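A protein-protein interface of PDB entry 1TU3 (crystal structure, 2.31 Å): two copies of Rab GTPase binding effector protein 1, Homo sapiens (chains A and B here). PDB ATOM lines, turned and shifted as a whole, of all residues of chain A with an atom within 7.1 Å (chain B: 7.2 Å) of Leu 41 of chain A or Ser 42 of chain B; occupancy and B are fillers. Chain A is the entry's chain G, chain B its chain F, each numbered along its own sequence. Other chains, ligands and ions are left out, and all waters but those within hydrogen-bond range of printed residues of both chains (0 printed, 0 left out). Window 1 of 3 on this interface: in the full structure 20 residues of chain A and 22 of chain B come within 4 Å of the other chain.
Among the printed residues, pairs that only touch across the chains: Phe 38 of chain A with Phe 38 of chain B (3.97 Å), Phe 38 of chain A with Val 39 of chain B (3.6 Å), Phe 38 of chain A with Ser 42 of chain B (3.5 Å), Val 39 of chain A with Phe 38 of chain B (3.9 Å), Leu 41 of chain A with Ser 42 of chain B (3.9 Å), Ser 42 of chain A with Phe 38 of chain B (3.3 Å), Ser 42 of chain A with Leu 41 of chain B (3.8 Å), Leu 45 of chain A with Ser 42 of chain B (3.8 Å), Leu 45 of chain A with Leu 45 of chain B (3.7 Å), Leu 45 of chain A with Gln 46 of chain B (3.7 Å) and Gln 46 of chain A with Leu 41 of chain B (3.97 Å).
Phe 38 of chain A touches its own counterpart, Phe 38 of chain B. Leu 45 of chain A touches Ser 42 of chain B, but with the chains exchanged Ser 42 of chain A does not touch Leu 45 of chain B (4.01 Å). Leu 45 of chain B touches its own counterpart, Leu 45 of chain A. Gln 46 of chain A touches Leu 41 of chain B, but with the chains exchanged Leu 41 of chain A does not touch Gln 46 of chain B (4.2 Å). Positions printed for both chains: 36, 37, 38, 39, 40, 41, 42, 43, 44, 45 and 46. Of the 11 pairs that touch across the chains among the printed residues, 8 have their exchanged pair printed and touching as well.
Printed residues of chain B within 4 Å of Leu 41 of chain A: Ser 42 (3.9 Å). Of the printed residues of chain A, Phe 38 of chain B touches Phe 38, Val 39 and Ser 42. Printed residues of chain A within 4 Å of Val 39 of chain B: Phe 38. Printed residues of chain A within 4 Å of Ser 42 of chain B: Phe 38, Leu 41 and Leu 45. Printed residues of chain A within 4 Å of Gln 46 of chain B: Leu 45 (3.7 Å). The nearest residue of chain B that does not touch Leu 41 of chain A is Gln 46 of chain B (4.2 Å). The nearest printed residue of chain A that does not touch Val 39 of chain B is Val 39 of chain A (6.5 Å).
The backbone carbonyl oxygen of Phe 38 of chain B sits close to the side-chain hydroxyl of Ser 42 of chain B, 3.5 Å away. OG of Ser 42 of chain B lies within hydrogen-bond range of O of Val 39 of chain B, 2.8 Å away. The side-chain amide oxygen (OE1) of Gln 46 of chain B sits close to the backbone carbonyl oxygen (O) of Ser 42 of chain B (3.4 Å). The backbone carbonyl oxygen (O) of Phe 38 of chain A lies within hydrogen-bond range of the side-chain hydroxyl (OG) of Ser 42 of chain A, at 3.3 Å. OG of Ser 42 of chain A is in hydrogen-bond range of O of Val 39 of chain A (2.9 Å). OE1 of Gln 46 of chain A lies close to O of Ser 42 of chain A.
Of the 13 printed residues of chain B, 6 touch a printed residue of chain A. Along chain B the printed residues that touch a printed residue of chain A span positions 38 to 46. Hydrophobic or aromatic side chains of chain A that line the printed part of chain B: Phe 38, Leu 41 and Leu 45. Among the printed residues, no Asp or Glu carboxylate lies within 4 Å of a Lys or Arg side-chain nitrogen of the other chain.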
ATOM      1  N   GLN A  35      -5.683  31.437  10.974  1.00  0.00           N
ATOM      2  CA  GLN A  35      -4.272  31.220  10.999  1.00  0.00           C
ATOM      3  C   GLN A  35      -3.801  30.881  12.408  1.00  0.00           C
ATOM      4  O   GLN A  35      -3.063  29.916  12.615  1.00  0.00           O
ATOM      5  CB  GLN A  35      -3.589  32.470  10.532  1.00  0.00           C
ATOM      6  CG  GLN A  35      -2.141  32.300  10.306  1.00  0.00           C
ATOM      7  CD  GLN A  35      -1.504  33.615   9.985  1.00  0.00           C
ATOM      8  OE1 GLN A  35      -1.181  34.385  10.877  1.00  0.00           O
ATOM      9  NE2 GLN A  35      -1.346  33.896   8.705  1.00  0.00           N
ATOM     10  N   ARG A  36      -4.221  31.702  13.366  1.00  0.00           N
ATOM     11  CA  ARG A  36      -3.827  31.554  14.752  1.00  0.00           C
ATOM     12  C   ARG A  36      -4.351  30.275  15.389  1.00  0.00           C
ATOM     13  O   ARG A  36      -3.686  29.688  16.247  1.00  0.00           O
ATOM     14  CB  ARG A  36      -4.297  32.756  15.563  1.00  0.00           C
ATOM     15  CG  ARG A  36      -3.437  34.000  15.296  1.00  0.00           C
ATOM     16  CD  ARG A  36      -3.669  35.092  16.347  1.00  0.00           C
ATOM     17  NE  ARG A  36      -5.042  35.601  16.332  1.00  0.00           N
ATOM     18  CZ  ARG A  36      -5.511  36.480  15.448  1.00  0.00           C
ATOM     19  NH1 ARG A  36      -4.716  36.962  14.496  1.00  0.00           N
ATOM     20  NH2 ARG A  36      -6.779  36.871  15.515  1.00  0.00           N
ATOM     21  N   ASP A  37      -5.547  29.859  14.971  1.00  0.00           N
ATOM     22  CA  ASP A  37      -6.133  28.605  15.414  1.00  0.00           C
ATOM     23  C   ASP A  37      -5.196  27.470  15.025  1.00  0.00           C
ATOM     24  O   ASP A  37      -4.948  26.558  15.805  1.00  0.00           O
ATOM     25  CB  ASP A  37      -7.479  28.324  14.746  1.00  0.00           C
ATOM     26  CG  ASP A  37      -8.648  29.134  15.333  1.00  0.00           C
ATOM     27  OD1 ASP A  37      -8.649  29.454  16.544  1.00  0.00           O
ATOM     28  OD2 ASP A  37      -9.597  29.408  14.562  1.00  0.00           O
ATOM     29  N   PHE A  38      -4.703  27.522  13.794  1.00  0.00           N
ATOM     30  CA  PHE A  38      -3.919  26.429  13.270  1.00  0.00           C
ATOM     31  C   PHE A  38      -2.486  26.481  13.787  1.00  0.00           C
ATOM     32  O   PHE A  38      -1.829  25.460  13.867  1.00  0.00           O
ATOM     33  CB  PHE A  38      -3.965  26.424  11.739  1.00  0.00           C
ATOM     34  CG  PHE A  38      -5.153  25.689  11.178  1.00  0.00           C
ATOM     35  CD1 PHE A  38      -5.167  24.285  11.111  1.00  0.00           C
ATOM     36  CD2 PHE A  38      -6.287  26.400  10.769  1.00  0.00           C
ATOM     37  CE1 PHE A  38      -6.306  23.602  10.646  1.00  0.00           C
ATOM     38  CE2 PHE A  38      -7.429  25.730  10.309  1.00  0.00           C
ATOM     39  CZ  PHE A  38      -7.445  24.334  10.246  1.00  0.00           C
ATOM     40  N   VAL A  39      -2.018  27.673  14.139  1.00  0.00           N
ATOM     41  CA  VAL A  39      -0.726  27.830  14.804  1.00  0.00           C
ATOM     42  C   VAL A  39      -0.795  27.216  16.200  1.00  0.00           C
ATOM     43  O   VAL A  39       0.070  26.424  16.577  1.00  0.00           O
ATOM     44  CB  VAL A  39      -0.316  29.310  14.965  1.00  0.00           C
ATOM     45  CG1 VAL A  39       1.012  29.410  15.740  1.00  0.00           C
ATOM     46  CG2 VAL A  39      -0.160  29.956  13.616  1.00  0.00           C
ATOM     47  N   LYS A  40      -1.822  27.578  16.964  1.00  0.00           N
ATOM     48  CA  LYS A  40      -2.006  26.978  18.278  1.00  0.00           C
ATOM     49  C   LYS A  40      -2.224  25.463  18.174  1.00  0.00           C
ATOM     50  O   LYS A  40      -1.668  24.710  18.980  1.00  0.00           O
ATOM     51  CB  LYS A  40      -3.171  27.647  19.016  1.00  0.00           C
ATOM     52  CG  LYS A  40      -2.951  29.142  19.234  1.00  0.00           C
ATOM     53  CD  LYS A  40      -3.727  29.695  20.420  1.00  0.00           C
ATOM     54  CE  LYS A  40      -5.226  29.588  20.220  1.00  0.00           C
ATOM     55  NZ  LYS A  40      -5.694  30.373  19.046  1.00  0.00           N
ATOM     56  N   LEU A  41      -2.987  25.025  17.163  1.00  0.00           N
ATOM     57  CA  LEU A  41      -3.188  23.596  16.912  1.00  0.00           C
ATOM     58  C   LEU A  41      -1.865  22.874  16.686  1.00  0.00           C
ATOM     59  O   LEU A  41      -1.628  21.809  17.256  1.00  0.00           O
ATOM     60  CB  LEU A  41      -4.067  23.350  15.684  1.00  0.00           C
ATOM     61  CG  LEU A  41      -5.065  22.160  15.721  1.00  0.00           C
ATOM     62  CD1 LEU A  41      -5.417  21.728  14.308  1.00  0.00           C
ATOM     63  CD2 LEU A  41      -4.514  20.985  16.468  1.00  0.00           C
ATOM     64  N   SER A  42      -1.009  23.430  15.834  1.00  0.00           N
ATOM     65  CA  SER A  42       0.235  22.733  15.550  1.00  0.00           C
ATOM     66  C   SER A  42       1.135  22.741  16.795  1.00  0.00           C
ATOM     67  O   SER A  42       1.720  21.717  17.121  1.00  0.00           O
ATOM     68  CB  SER A  42       0.960  23.350  14.337  1.00  0.00           C
ATOM     69  OG  SER A  42       1.336  24.679  14.613  1.00  0.00           O
ATOM     70  N   GLN A  43       1.231  23.881  17.490  1.00  0.00           N
ATOM     71  CA  GLN A  43       2.041  23.930  18.701  1.00  0.00           C
ATOM     72  C   GLN A  43       1.632  22.827  19.695  1.00  0.00           C
ATOM     73  O   GLN A  43       2.481  22.184  20.284  1.00  0.00           O
ATOM     74  CB  GLN A  43       1.937  25.287  19.391  1.00  0.00           C
ATOM     75  CG  GLN A  43       2.524  26.425  18.623  1.00  0.00           C
ATOM     76  CD  GLN A  43       2.284  27.772  19.305  1.00  0.00           C
ATOM     77  OE1 GLN A  43       1.178  28.054  19.787  1.00  0.00           O
ATOM     78  NE2 GLN A  43       3.315  28.611  19.336  1.00  0.00           N
ATOM     79  N   THR A  44       0.331  22.638  19.868  1.00  0.00           N
ATOM     80  CA  THR A  44      -0.164  21.650  20.792  1.00  0.00           C
ATOM     81  C   THR A  44       0.225  20.247  20.349  1.00  0.00           C
ATOM     82  O   THR A  44       0.672  19.435  21.155  1.00  0.00           O
ATOM     83  CB  THR A  44      -1.687  21.772  20.935  1.00  0.00           C
ATOM     84  OG1 THR A  44      -1.980  22.913  21.752  1.00  0.00           O
ATOM     85  CG2 THR A  44      -2.289  20.515  21.579  1.00  0.00           C
ATOM     86  N   LEU A  45       0.065  19.975  19.060  1.00  0.00           N
ATOM     87  CA  LEU A  45       0.412  18.673  18.519  1.00  0.00           C
ATOM     88  C   LEU A  45       1.900  18.372  18.656  1.00  0.00           C
ATOM     89  O   LEU A  45       2.284  17.253  19.008  1.00  0.00           O
ATOM     90  CB  LEU A  45       0.006  18.588  17.051  1.00  0.00           C
ATOM     91  CG  LEU A  45      -1.483  18.689  16.764  1.00  0.00           C
ATOM     92  CD1 LEU A  45      -1.694  18.804  15.255  1.00  0.00           C
ATOM     93  CD2 LEU A  45      -2.193  17.462  17.340  1.00  0.00           C
ATOM     94  N   GLN A  46       2.738  19.362  18.366  1.00  0.00           N
ATOM     95  CA  GLN A  46       4.176  19.170  18.491  1.00  0.00           C
ATOM     96  C   GLN A  46       4.635  18.901  19.942  1.00  0.00           C
ATOM     97  O   GLN A  46       5.453  18.010  20.174  1.00  0.00           O
ATOM     98  CB  GLN A  46       4.922  20.378  17.903  1.00  0.00           C
ATOM     99  CG  GLN A  46       4.793  20.450  16.393  1.00  0.00           C
ATOM    100  CD  GLN A  46       5.144  21.804  15.800  1.00  0.00           C
ATOM    101  OE1 GLN A  46       4.904  22.864  16.418  1.00  0.00           O
ATOM    102  NE2 GLN A  46       5.698  21.786  14.602  1.00  0.00           N
ATOM    103  N   LYS A  69      -6.232  19.151  24.583  1.00  0.00           N
ATOM    104  CA  LYS A  69      -5.662  20.037  23.571  1.00  0.00           C
ATOM    105  C   LYS A  69      -6.445  21.348  23.502  1.00  0.00           C
ATOM    106  O   LYS A  69      -7.392  21.520  24.305  1.00  0.00           O
ATOM    107  CB  LYS A  69      -5.677  19.367  22.192  1.00  0.00           C
ATOM    108  CG  LYS A  69      -5.010  18.004  22.143  1.00  0.00           C
ATOM    109  CD  LYS A  69      -5.978  16.911  22.564  1.00  0.00           C
ATOM    110  CE  LYS A  69      -5.298  15.554  22.663  1.00  0.00           C
ATOM    111  NZ  LYS A  69      -4.383  15.484  23.829  1.00  0.00           N
ATOM    112  N   ARG B  36      -2.250  28.407   5.278  1.00  0.00           N
ATOM    113  CA  ARG B  36      -2.237  27.105   4.630  1.00  0.00           C
ATOM    114  C   ARG B  36      -0.987  26.316   4.994  1.00  0.00           C
ATOM    115  O   ARG B  36      -1.016  25.083   5.058  1.00  0.00           O
ATOM    116  CB  ARG B  36      -2.383  27.263   3.106  1.00  0.00           C
ATOM    117  CG  ARG B  36      -3.801  27.659   2.786  1.00  0.00           C
ATOM    118  CD  ARG B  36      -4.225  27.498   1.345  1.00  0.00           C
ATOM    119  NE  ARG B  36      -3.677  28.586   0.564  1.00  0.00           N
ATOM    120  CZ  ARG B  36      -2.463  28.569   0.056  1.00  0.00           C
ATOM    121  NH1 ARG B  36      -1.712  27.494   0.240  1.00  0.00           N
ATOM    122  NH2 ARG B  36      -1.980  29.646  -0.551  1.00  0.00           N
ATOM    123  N   ASP B  37       0.109  27.022   5.253  1.00  0.00           N
ATOM    124  CA  ASP B  37       1.277  26.320   5.714  1.00  0.00           C
ATOM    125  C   ASP B  37       0.910  25.593   7.005  1.00  0.00           C
ATOM    126  O   ASP B  37       1.294  24.455   7.175  1.00  0.00           O
ATOM    127  CB  ASP B  37       2.456  27.251   5.978  1.00  0.00           C
ATOM    128  CG  ASP B  37       3.050  27.837   4.702  1.00  0.00           C
ATOM    129  OD1 ASP B  37       3.070  27.138   3.659  1.00  0.00           O
ATOM    130  OD2 ASP B  37       3.511  29.000   4.769  1.00  0.00           O
ATOM    131  N   PHE B  38       0.166  26.246   7.898  1.00  0.00           N
ATOM    132  CA  PHE B  38      -0.033  25.644   9.194  1.00  0.00           C
ATOM    133  C   PHE B  38      -1.157  24.600   9.129  1.00  0.00           C
ATOM    134  O   PHE B  38      -1.090  23.595   9.810  1.00  0.00           O
ATOM    135  CB  PHE B  38      -0.283  26.694  10.274  1.00  0.00           C
ATOM    136  CG  PHE B  38       0.977  27.265  10.842  1.00  0.00           C
ATOM    137  CD1 PHE B  38       1.594  28.382  10.255  1.00  0.00           C
ATOM    138  CD2 PHE B  38       1.596  26.652  11.934  1.00  0.00           C
ATOM    139  CE1 PHE B  38       2.811  28.863  10.751  1.00  0.00           C
ATOM    140  CE2 PHE B  38       2.815  27.122  12.446  1.00  0.00           C
ATOM    141  CZ  PHE B  38       3.430  28.234  11.853  1.00  0.00           C
ATOM    142  N   VAL B  39      -2.151  24.808   8.267  1.00  0.00           N
ATOM    143  CA  VAL B  39      -3.102  23.738   7.989  1.00  0.00           C
ATOM    144  C   VAL B  39      -2.408  22.461   7.532  1.00  0.00           C
ATOM    145  O   VAL B  39      -2.648  21.407   8.096  1.00  0.00           O
ATOM    146  CB  VAL B  39      -4.123  24.111   6.935  1.00  0.00           C
ATOM    147  CG1 VAL B  39      -4.835  22.852   6.419  1.00  0.00           C
ATOM    148  CG2 VAL B  39      -5.155  25.070   7.549  1.00  0.00           C
ATOM    149  N   LYS B  40      -1.551  22.556   6.520  1.00  0.00           N
ATOM    150  CA  LYS B  40      -0.793  21.395   6.066  1.00  0.00           C
ATOM    151  C   LYS B  40       0.018  20.776   7.187  1.00  0.00           C
ATOM    152  O   LYS B  40      -0.053  19.572   7.421  1.00  0.00           O
ATOM    153  CB  LYS B  40       0.165  21.757   4.938  1.00  0.00           C
ATOM    154  CG  LYS B  40      -0.310  21.327   3.585  1.00  0.00           C
ATOM    155  CD  LYS B  40      -1.083  22.423   2.896  1.00  0.00           C
ATOM    156  CE  LYS B  40      -0.250  23.084   1.804  1.00  0.00           C
ATOM    157  NZ  LYS B  40       1.005  23.724   2.289  1.00  0.00           N
ATOM    158  N   LEU B  41       0.804  21.617   7.855  1.00  0.00           N
ATOM    159  CA  LEU B  41       1.586  21.184   8.988  1.00  0.00           C
ATOM    160  C   LEU B  41       0.727  20.432  10.029  1.00  0.00           C
ATOM    161  O   LEU B  41       1.133  19.390  10.496  1.00  0.00           O
ATOM    162  CB  LEU B  41       2.292  22.359   9.640  1.00  0.00           C
ATOM    163  CG  LEU B  41       3.021  22.002  10.949  1.00  0.00           C
ATOM    164  CD1 LEU B  41       4.106  20.951  10.713  1.00  0.00           C
ATOM    165  CD2 LEU B  41       3.599  23.237  11.565  1.00  0.00           C
ATOM    166  N   SER B  42      -0.453  20.952  10.372  1.00  0.00           N
ATOM    167  CA  SER B  42      -1.316  20.273  11.332  1.00  0.00           C
ATOM    168  C   SER B  42      -1.810  18.920  10.797  1.00  0.00           C
ATOM    169  O   SER B  42      -1.970  17.981  11.565  1.00  0.00           O
ATOM    170  CB  SER B  42      -2.508  21.149  11.731  1.00  0.00           C
ATOM    171  OG  SER B  42      -3.501  21.237  10.715  1.00  0.00           O
ATOM    172  N   GLN B  43      -2.033  18.822   9.485  1.00  0.00           N
ATOM    173  CA  GLN B  43      -2.482  17.586   8.889  1.00  0.00           C
ATOM    174  C   GLN B  43      -1.442  16.489   9.019  1.00  0.00           C
ATOM    175  O   GLN B  43      -1.781  15.336   9.288  1.00  0.00           O
ATOM    176  CB  GLN B  43      -2.823  17.786   7.415  1.00  0.00           C
ATOM    177  CG  GLN B  43      -4.181  18.428   7.197  1.00  0.00           C
ATOM    178  CD  GLN B  43      -4.398  18.827   5.746  1.00  0.00           C
ATOM    179  OE1 GLN B  43      -3.450  19.065   5.002  1.00  0.00           O
ATOM    180  NE2 GLN B  43      -5.651  18.923   5.347  1.00  0.00           N
ATOM    181  N   THR B  44      -0.180  16.865   8.842  1.00  0.00           N
ATOM    182  CA  THR B  44       0.926  15.927   8.945  1.00  0.00           C
ATOM    183  C   THR B  44       1.070  15.436  10.402  1.00  0.00           C
ATOM    184  O   THR B  44       1.074  14.232  10.653  1.00  0.00           O
ATOM    185  CB  THR B  44       2.260  16.582   8.524  1.00  0.00           C
ATOM    186  OG1 THR B  44       2.160  17.048   7.178  1.00  0.00           O
ATOM    187  CG2 THR B  44       3.371  15.599   8.628  1.00  0.00           C
ATOM    188  N   LEU B  45       1.178  16.378  11.341  1.00  0.00           N
ATOM    189  CA  LEU B  45       1.199  16.059  12.767  1.00  0.00           C
ATOM    190  C   LEU B  45       0.031  15.144  13.225  1.00  0.00           C
ATOM    191  O   LEU B  45       0.248  14.149  13.917  1.00  0.00           O
ATOM    192  CB  LEU B  45       1.205  17.335  13.584  1.00  0.00           C
ATOM    193  CG  LEU B  45       2.481  18.170  13.713  1.00  0.00           C
ATOM    194  CD1 LEU B  45       3.551  17.687  12.770  1.00  0.00           C
ATOM    195  CD2 LEU B  45       2.144  19.623  13.468  1.00  0.00           C
ATOM    196  N   GLN B  46      -1.194  15.453  12.814  1.00  0.00           N
ATOM    197  CA  GLN B  46      -2.306  14.574  13.133  1.00  0.00           C
ATOM    198  C   GLN B  46      -2.186  13.161  12.531  1.00  0.00           C
ATOM    199  O   GLN B  46      -2.584  12.208  13.167  1.00  0.00           O
ATOM    200  CB  GLN B  46      -3.622  15.223  12.703  1.00  0.00           C
ATOM    201  CG  GLN B  46      -3.948  16.456  13.525  1.00  0.00           C
ATOM    202  CD  GLN B  46      -5.145  17.202  12.997  1.00  0.00           C
ATOM    203  OE1 GLN B  46      -5.290  17.395  11.772  1.00  0.00           O
ATOM    204  NE2 GLN B  46      -6.011  17.631  13.899  1.00  0.00           N
ATOM    205  N   VAL B  47      -1.654  13.028  11.314  1.00  0.00           N
ATOM    206  CA  VAL B  47      -1.514  11.706  10.697  1.00  0.00           C
ATOM    207  C   VAL B  47      -0.451  10.918  11.469  1.00  0.00           C
ATOM    208  O   VAL B  47      -0.623   9.751  11.783  1.00  0.00           O
ATOM    209  CB  VAL B  47      -1.118  11.801   9.211  1.00  0.00           C
ATOM    210  CG1 VAL B  47      -0.599  10.450   8.689  1.00  0.00           C
ATOM    211  CG2 VAL B  47      -2.332  12.234   8.393  1.00  0.00           C
ATOM    212  N   GLN B  48       0.638  11.583  11.790  1.00  0.00           N
ATOM    213  CA  GLN B  48       1.654  10.980  12.579  1.00  0.00           C
ATOM    214  C   GLN B  48       1.131  10.563  13.972  1.00  0.00           C
ATOM    215  O   GLN B  48       1.354   9.440  14.405  1.00  0.00           O
ATOM    216  CB  GLN B  48       2.834  11.937  12.681  1.00  0.00           C
ATOM    217  CG  GLN B  48       3.971  11.429  13.501  1.00  0.00           C
ATOM    218  CD  GLN B  48       5.259  12.099  13.141  1.00  0.00           C
ATOM    219  OE1 GLN B  48       5.327  13.319  13.038  1.00  0.00           O
ATOM    220  NE2 GLN B  48       6.306  11.298  12.945  1.00  0.00           N
